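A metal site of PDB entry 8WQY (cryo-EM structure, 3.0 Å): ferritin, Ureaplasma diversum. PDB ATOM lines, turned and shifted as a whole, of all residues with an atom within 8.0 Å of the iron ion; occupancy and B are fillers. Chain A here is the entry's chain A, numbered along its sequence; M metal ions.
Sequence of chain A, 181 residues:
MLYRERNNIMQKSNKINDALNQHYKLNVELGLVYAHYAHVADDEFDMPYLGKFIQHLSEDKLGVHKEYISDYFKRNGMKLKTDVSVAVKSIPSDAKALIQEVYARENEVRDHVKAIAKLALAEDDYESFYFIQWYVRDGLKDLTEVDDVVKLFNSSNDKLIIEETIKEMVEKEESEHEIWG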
ATOM      1  N   ASN A  27       3.756  17.223  13.320  1.00  0.00           N
ATOM      2  CA  ASN A  27       2.618  17.929  13.906  1.00  0.00           C
ATOM      3  C   ASN A  27       2.644  19.408  13.550  1.00  0.00           C
ATOM      4  O   ASN A  27       1.600  19.994  13.218  1.00  0.00           O
ATOM      5  CB  ASN A  27       2.615  17.739  15.422  1.00  0.00           C
ATOM      6  CG  ASN A  27       1.729  16.598  15.856  1.00  0.00           C
ATOM      7  OD1 ASN A  27       0.597  16.466  15.399  1.00  0.00           O
ATOM      8  ND2 ASN A  27       2.243  15.773  16.750  1.00  0.00           N
ATOM      9  N   HIS A  56     -10.174  24.705  14.784  1.00  0.00           N
ATOM     10  CA  HIS A  56      -9.990  24.008  16.044  1.00  0.00           C
ATOM     11  C   HIS A  56      -8.999  22.863  15.888  1.00  0.00           C
ATOM     12  O   HIS A  56      -8.152  22.650  16.769  1.00  0.00           O
ATOM     13  CB  HIS A  56     -11.334  23.483  16.558  1.00  0.00           C
ATOM     14  CG  HIS A  56     -12.168  24.544  17.212  1.00  0.00           C
ATOM     15  ND1 HIS A  56     -11.708  25.320  18.250  1.00  0.00           N
ATOM     16  CD2 HIS A  56     -13.429  24.958  16.952  1.00  0.00           C
ATOM     17  CE1 HIS A  56     -12.653  26.165  18.614  1.00  0.00           C
ATOM     18  NE2 HIS A  56     -13.709  25.971  17.845  1.00  0.00           N
ATOM     19  N   LEU A  57      -9.074  22.136  14.783  1.00  0.00           N
ATOM     20  CA  LEU A  57      -8.084  21.074  14.551  1.00  0.00           C
ATOM     21  C   LEU A  57      -6.671  21.625  14.488  1.00  0.00           C
ATOM     22  O   LEU A  57      -5.739  21.048  15.069  1.00  0.00           O
ATOM     23  CB  LEU A  57      -8.412  20.309  13.271  1.00  0.00           C
ATOM     24  CG  LEU A  57      -9.530  19.278  13.366  1.00  0.00           C
ATOM     25  CD1 LEU A  57      -9.734  18.622  12.016  1.00  0.00           C
ATOM     26  CD2 LEU A  57      -9.178  18.246  14.410  1.00  0.00           C
ATOM     27  N   ASP A  60      -5.401  22.618  17.893  1.00  0.00           N
ATOM     28  CA  ASP A  60      -5.040  21.416  18.642  1.00  0.00           C
ATOM     29  C   ASP A  60      -3.679  20.893  18.212  1.00  0.00           C
ATOM     30  O   ASP A  60      -2.827  20.571  19.060  1.00  0.00           O
ATOM     31  CB  ASP A  60      -6.105  20.349  18.473  1.00  0.00           C
ATOM     32  CG  ASP A  60      -6.272  19.492  19.698  1.00  0.00           C
ATOM     33  OD1 ASP A  60      -5.548  19.734  20.690  1.00  0.00           O
ATOM     34  OD2 ASP A  60      -7.121  18.584  19.682  1.00  0.00           O
ATOM     35  N   LYS A  61      -3.438  20.794  16.905  1.00  0.00           N
ATOM     36  CA  LYS A  61      -2.177  20.241  16.439  1.00  0.00           C
ATOM     37  C   LYS A  61      -0.988  21.118  16.792  1.00  0.00           C
ATOM     38  O   LYS A  61       0.129  20.626  16.932  1.00  0.00           O
ATOM     39  CB  LYS A  61      -2.228  20.008  14.929  1.00  0.00           C
ATOM     40  CG  LYS A  61      -3.099  18.848  14.506  1.00  0.00           C
ATOM     41  CD  LYS A  61      -2.510  17.529  14.946  1.00  0.00           C
ATOM     42  CE  LYS A  61      -3.246  16.366  14.308  1.00  0.00           C
ATOM     43  NZ  LYS A  61      -4.664  16.306  14.725  1.00  0.00           N
ATOM     44  N   VAL A  64      -1.128  21.457  22.457  1.00  0.00           N
ATOM     45  CA  VAL A  64      -0.714  20.403  23.364  1.00  0.00           C
ATOM     46  C   VAL A  64      -0.008  19.276  22.627  1.00  0.00           C
ATOM     47  O   VAL A  64       0.972  18.720  23.134  1.00  0.00           O
ATOM     48  CB  VAL A  64      -1.913  19.877  24.173  1.00  0.00           C
ATOM     49  CG1 VAL A  64      -2.447  20.975  25.066  1.00  0.00           C
ATOM     50  CG2 VAL A  64      -3.001  19.403  23.256  1.00  0.00           C
ATOM     51  N   HIS A  65      -0.435  18.962  21.406  1.00  0.00           N
ATOM     52  CA  HIS A  65       0.142  17.858  20.656  1.00  0.00           C
ATOM     53  C   HIS A  65       1.652  17.991  20.481  1.00  0.00           C
ATOM     54  O   HIS A  65       2.301  17.010  20.089  1.00  0.00           O
ATOM     55  CB  HIS A  65      -0.515  17.736  19.288  1.00  0.00           C
ATOM     56  CG  HIS A  65      -1.774  16.925  19.279  1.00  0.00           C
ATOM     57  ND1 HIS A  65      -1.871  15.720  18.610  1.00  0.00           N
ATOM     58  CD2 HIS A  65      -2.983  17.145  19.832  1.00  0.00           C
ATOM     59  CE1 HIS A  65      -3.096  15.233  18.764  1.00  0.00           C
ATOM     60  NE2 HIS A  65      -3.785  16.082  19.492  1.00  0.00           N
ATOM     61  N   GLU A 106      -5.168  12.526   8.819  1.00  0.00           N
ATOM     62  CA  GLU A 106      -5.351  11.952  10.151  1.00  0.00           C
ATOM     63  C   GLU A 106      -5.097  10.442  10.132  1.00  0.00           C
ATOM     64  O   GLU A 106      -4.435   9.895  11.030  1.00  0.00           O
ATOM     65  CB  GLU A 106      -6.763  12.265  10.655  1.00  0.00           C
ATOM     66  CG  GLU A 106      -6.881  13.574  11.417  1.00  0.00           C
ATOM     67  CD  GLU A 106      -6.159  13.578  12.750  1.00  0.00           C
ATOM     68  OE1 GLU A 106      -6.163  14.617  13.434  1.00  0.00           O
ATOM     69  OE2 GLU A 106      -5.595  12.526  13.146  1.00  0.00           O
ATOM     70  N   TRP A 134      -1.145   8.056  25.290  1.00  0.00           N
ATOM     71  CA  TRP A 134      -2.037   9.193  25.094  1.00  0.00           C
ATOM     72  C   TRP A 134      -2.274   9.457  23.620  1.00  0.00           C
ATOM     73  O   TRP A 134      -3.408   9.680  23.184  1.00  0.00           O
ATOM     74  CB  TRP A 134      -1.452  10.434  25.774  1.00  0.00           C
ATOM     75  CG  TRP A 134      -2.440  11.538  25.972  1.00  0.00           C
ATOM     76  CD1 TRP A 134      -3.265  11.715  27.042  1.00  0.00           C
ATOM     77  CD2 TRP A 134      -2.688  12.642  25.088  1.00  0.00           C
ATOM     78  NE1 TRP A 134      -4.019  12.846  26.876  1.00  0.00           N
ATOM     79  CE2 TRP A 134      -3.691  13.435  25.687  1.00  0.00           C
ATOM     80  CE3 TRP A 134      -2.170  13.030  23.855  1.00  0.00           C
ATOM     81  CZ2 TRP A 134      -4.176  14.588  25.095  1.00  0.00           C
ATOM     82  CZ3 TRP A 134      -2.660  14.176  23.267  1.00  0.00           C
ATOM     83  CH2 TRP A 134      -3.646  14.944  23.883  1.00  0.00           C
ATOM     84  N   TYR A 135      -1.204   9.444  22.829  1.00  0.00           N
ATOM     85  CA  TYR A 135      -1.339   9.673  21.389  1.00  0.00           C
ATOM     86  C   TYR A 135      -2.074   8.531  20.721  1.00  0.00           C
ATOM     87  O   TYR A 135      -2.873   8.739  19.808  1.00  0.00           O
ATOM     88  CB  TYR A 135       0.034   9.882  20.765  1.00  0.00           C
ATOM     89  CG  TYR A 135       0.687  11.183  21.165  1.00  0.00           C
ATOM     90  CD1 TYR A 135       1.183  11.369  22.449  1.00  0.00           C
ATOM     91  CD2 TYR A 135       0.806  12.226  20.271  1.00  0.00           C
ATOM     92  CE1 TYR A 135       1.766  12.554  22.821  1.00  0.00           C
ATOM     93  CE2 TYR A 135       1.394  13.411  20.627  1.00  0.00           C
ATOM     94  CZ  TYR A 135       1.878  13.572  21.900  1.00  0.00           C
ATOM     95  OH  TYR A 135       2.466  14.758  22.255  1.00  0.00           O
ATOM     96  N   ARG A 137      -4.485   6.895  21.914  1.00  0.00           N
ATOM     97  CA  ARG A 137      -5.917   7.097  22.109  1.00  0.00           C
ATOM     98  C   ARG A 137      -6.447   8.313  21.338  1.00  0.00           C
ATOM     99  O   ARG A 137      -7.518   8.252  20.702  1.00  0.00           O
ATOM    100  CB  ARG A 137      -6.225   7.240  23.590  1.00  0.00           C
ATOM    101  CG  ARG A 137      -7.682   7.399  23.908  1.00  0.00           C
ATOM    102  CD  ARG A 137      -8.008   8.816  24.327  1.00  0.00           C
ATOM    103  NE  ARG A 137      -7.267   9.208  25.512  1.00  0.00           N
ATOM    104  CZ  ARG A 137      -6.982  10.459  25.832  1.00  0.00           C
ATOM    105  NH1 ARG A 137      -7.369  11.443  25.031  1.00  0.00           N
ATOM    106  NH2 ARG A 137      -6.305  10.732  26.925  1.00  0.00           N
ATOM    107  N   ASP A 138      -5.709   9.423  21.382  1.00  0.00           N
ATOM    108  CA  ASP A 138      -6.209  10.645  20.787  1.00  0.00           C
ATOM    109  C   ASP A 138      -6.268  10.562  19.266  1.00  0.00           C
ATOM    110  O   ASP A 138      -7.101  11.230  18.649  1.00  0.00           O
ATOM    111  CB  ASP A 138      -5.355  11.831  21.217  1.00  0.00           C
ATOM    112  CG  ASP A 138      -6.098  13.133  21.120  1.00  0.00           C
ATOM    113  OD1 ASP A 138      -6.870  13.452  22.042  1.00  0.00           O
ATOM    114  OD2 ASP A 138      -5.917  13.843  20.098  1.00  0.00           O
ATOM    115  N   GLY A 139      -5.398   9.755  18.652  1.00  0.00           N
ATOM    116  CA  GLY A 139      -5.499   9.566  17.217  1.00  0.00           C
ATOM    117  C   GLY A 139      -6.857   9.049  16.804  1.00  0.00           C
ATOM    118  O   GLY A 139      -7.515   9.598  15.914  1.00  0.00           O
ATOM    119  N   LEU A 140      -7.316   7.984  17.469  1.00  0.00           N
ATOM    120  CA  LEU A 140      -8.614   7.412  17.148  1.00  0.00           C
ATOM    121  C   LEU A 140      -9.744   8.377  17.482  1.00  0.00           C
ATOM    122  O   LEU A 140     -10.725   8.474  16.742  1.00  0.00           O
ATOM    123  CB  LEU A 140      -8.807   6.095  17.886  1.00  0.00           C
ATOM    124  CG  LEU A 140     -10.124   5.382  17.591  1.00  0.00           C
ATOM    125  CD1 LEU A 140     -10.250   5.084  16.120  1.00  0.00           C
ATOM    126  CD2 LEU A 140     -10.177   4.103  18.372  1.00  0.00           C
ATOM    127  N   LYS A 141      -9.633   9.105  18.600  1.00  0.00           N
ATOM    128  CA  LYS A 141     -10.655  10.091  18.917  1.00  0.00           C
ATOM    129  C   LYS A 141     -10.810  11.110  17.788  1.00  0.00           C
ATOM    130  O   LYS A 141     -11.921  11.334  17.262  1.00  0.00           O
ATOM    131  CB  LYS A 141     -10.334  10.813  20.224  1.00  0.00           C
ATOM    132  CG  LYS A 141     -11.317  11.922  20.528  1.00  0.00           C
ATOM    133  CD  LYS A 141     -11.049  12.555  21.874  1.00  0.00           C
ATOM    134  CE  LYS A 141     -12.250  13.359  22.350  1.00  0.00           C
ATOM    135  NZ  LYS A 141     -12.009  14.007  23.676  1.00  0.00           N
ATOM    136  N   ASP A 142      -9.705  11.742  17.395  1.00  0.00           N
ATOM    137  CA  ASP A 142      -9.762  12.771  16.355  1.00  0.00           C
ATOM    138  C   ASP A 142     -10.243  12.203  15.034  1.00  0.00           C
ATOM    139  O   ASP A 142     -11.009  12.852  14.311  1.00  0.00           O
ATOM    140  CB  ASP A 142      -8.390  13.433  16.202  1.00  0.00           C
ATOM    141  CG  ASP A 142      -8.025  14.303  17.388  1.00  0.00           C
ATOM    142  OD1 ASP A 142      -8.913  14.601  18.208  1.00  0.00           O
ATOM    143  OD2 ASP A 142      -6.837  14.692  17.499  1.00  0.00           O
ATOM    144  N   LEU A 143      -9.810  10.985  14.689  1.00  0.00           N
ATOM    145  CA  LEU A 143     -10.226  10.412  13.421  1.00  0.00           C
ATOM    146  C   LEU A 143     -11.717  10.151  13.385  1.00  0.00           C
ATOM    147  O   LEU A 143     -12.379  10.404  12.369  1.00  0.00           O
ATOM    148  CB  LEU A 143      -9.443   9.131  13.140  1.00  0.00           C
ATOM    149  CG  LEU A 143      -9.717   8.497  11.786  1.00  0.00           C
ATOM    150  CD1 LEU A 143      -8.422   8.088  11.134  1.00  0.00           C
ATOM    151  CD2 LEU A 143     -10.621   7.290  11.950  1.00  0.00           C
ATOM    152  N   GLU A 145     -13.997  11.823  15.090  1.00  0.00           N
ATOM    153  CA  GLU A 145     -14.710  13.097  15.040  1.00  0.00           C
ATOM    154  C   GLU A 145     -14.517  13.826  13.723  1.00  0.00           C
ATOM    155  O   GLU A 145     -15.250  14.791  13.461  1.00  0.00           O
ATOM    156  CB  GLU A 145     -14.304  13.997  16.204  1.00  0.00           C
ATOM    157  CG  GLU A 145     -13.147  14.918  15.906  1.00  0.00           C
ATOM    158  CD  GLU A 145     -12.739  15.726  17.110  1.00  0.00           C
ATOM    159  OE1 GLU A 145     -13.386  15.585  18.166  1.00  0.00           O
ATOM    160  OE2 GLU A 145     -11.765  16.509  17.001  1.00  0.00           O
HETATM  161 FE    FE M   1      -5.716  15.448  18.932  1.00  0.00          FE
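The side-chain carboxylate (OD2) of Asp 142 sits close to the side-chain amino group (NZ) of Lys 61, 3.9 Å away.
The side-chain carboxylate (OD1) of Asp 138 lies within salt-bridge range of the guanidinium group (NH1) of Arg 137.
The side-chain hydroxyl (OH) of Tyr 135 is in hydrogen-bond range of the backbone carbonyl oxygen (O) of His 65, 3.1 Å away.
Asp 60 touches the iron ion.
The iron ion is bound by the side-chain carboxylate (OD2) of Asp 142, the side-chain carboxylate (OD2) of Asp 138 and a ring nitrogen (NE2) of His 65.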
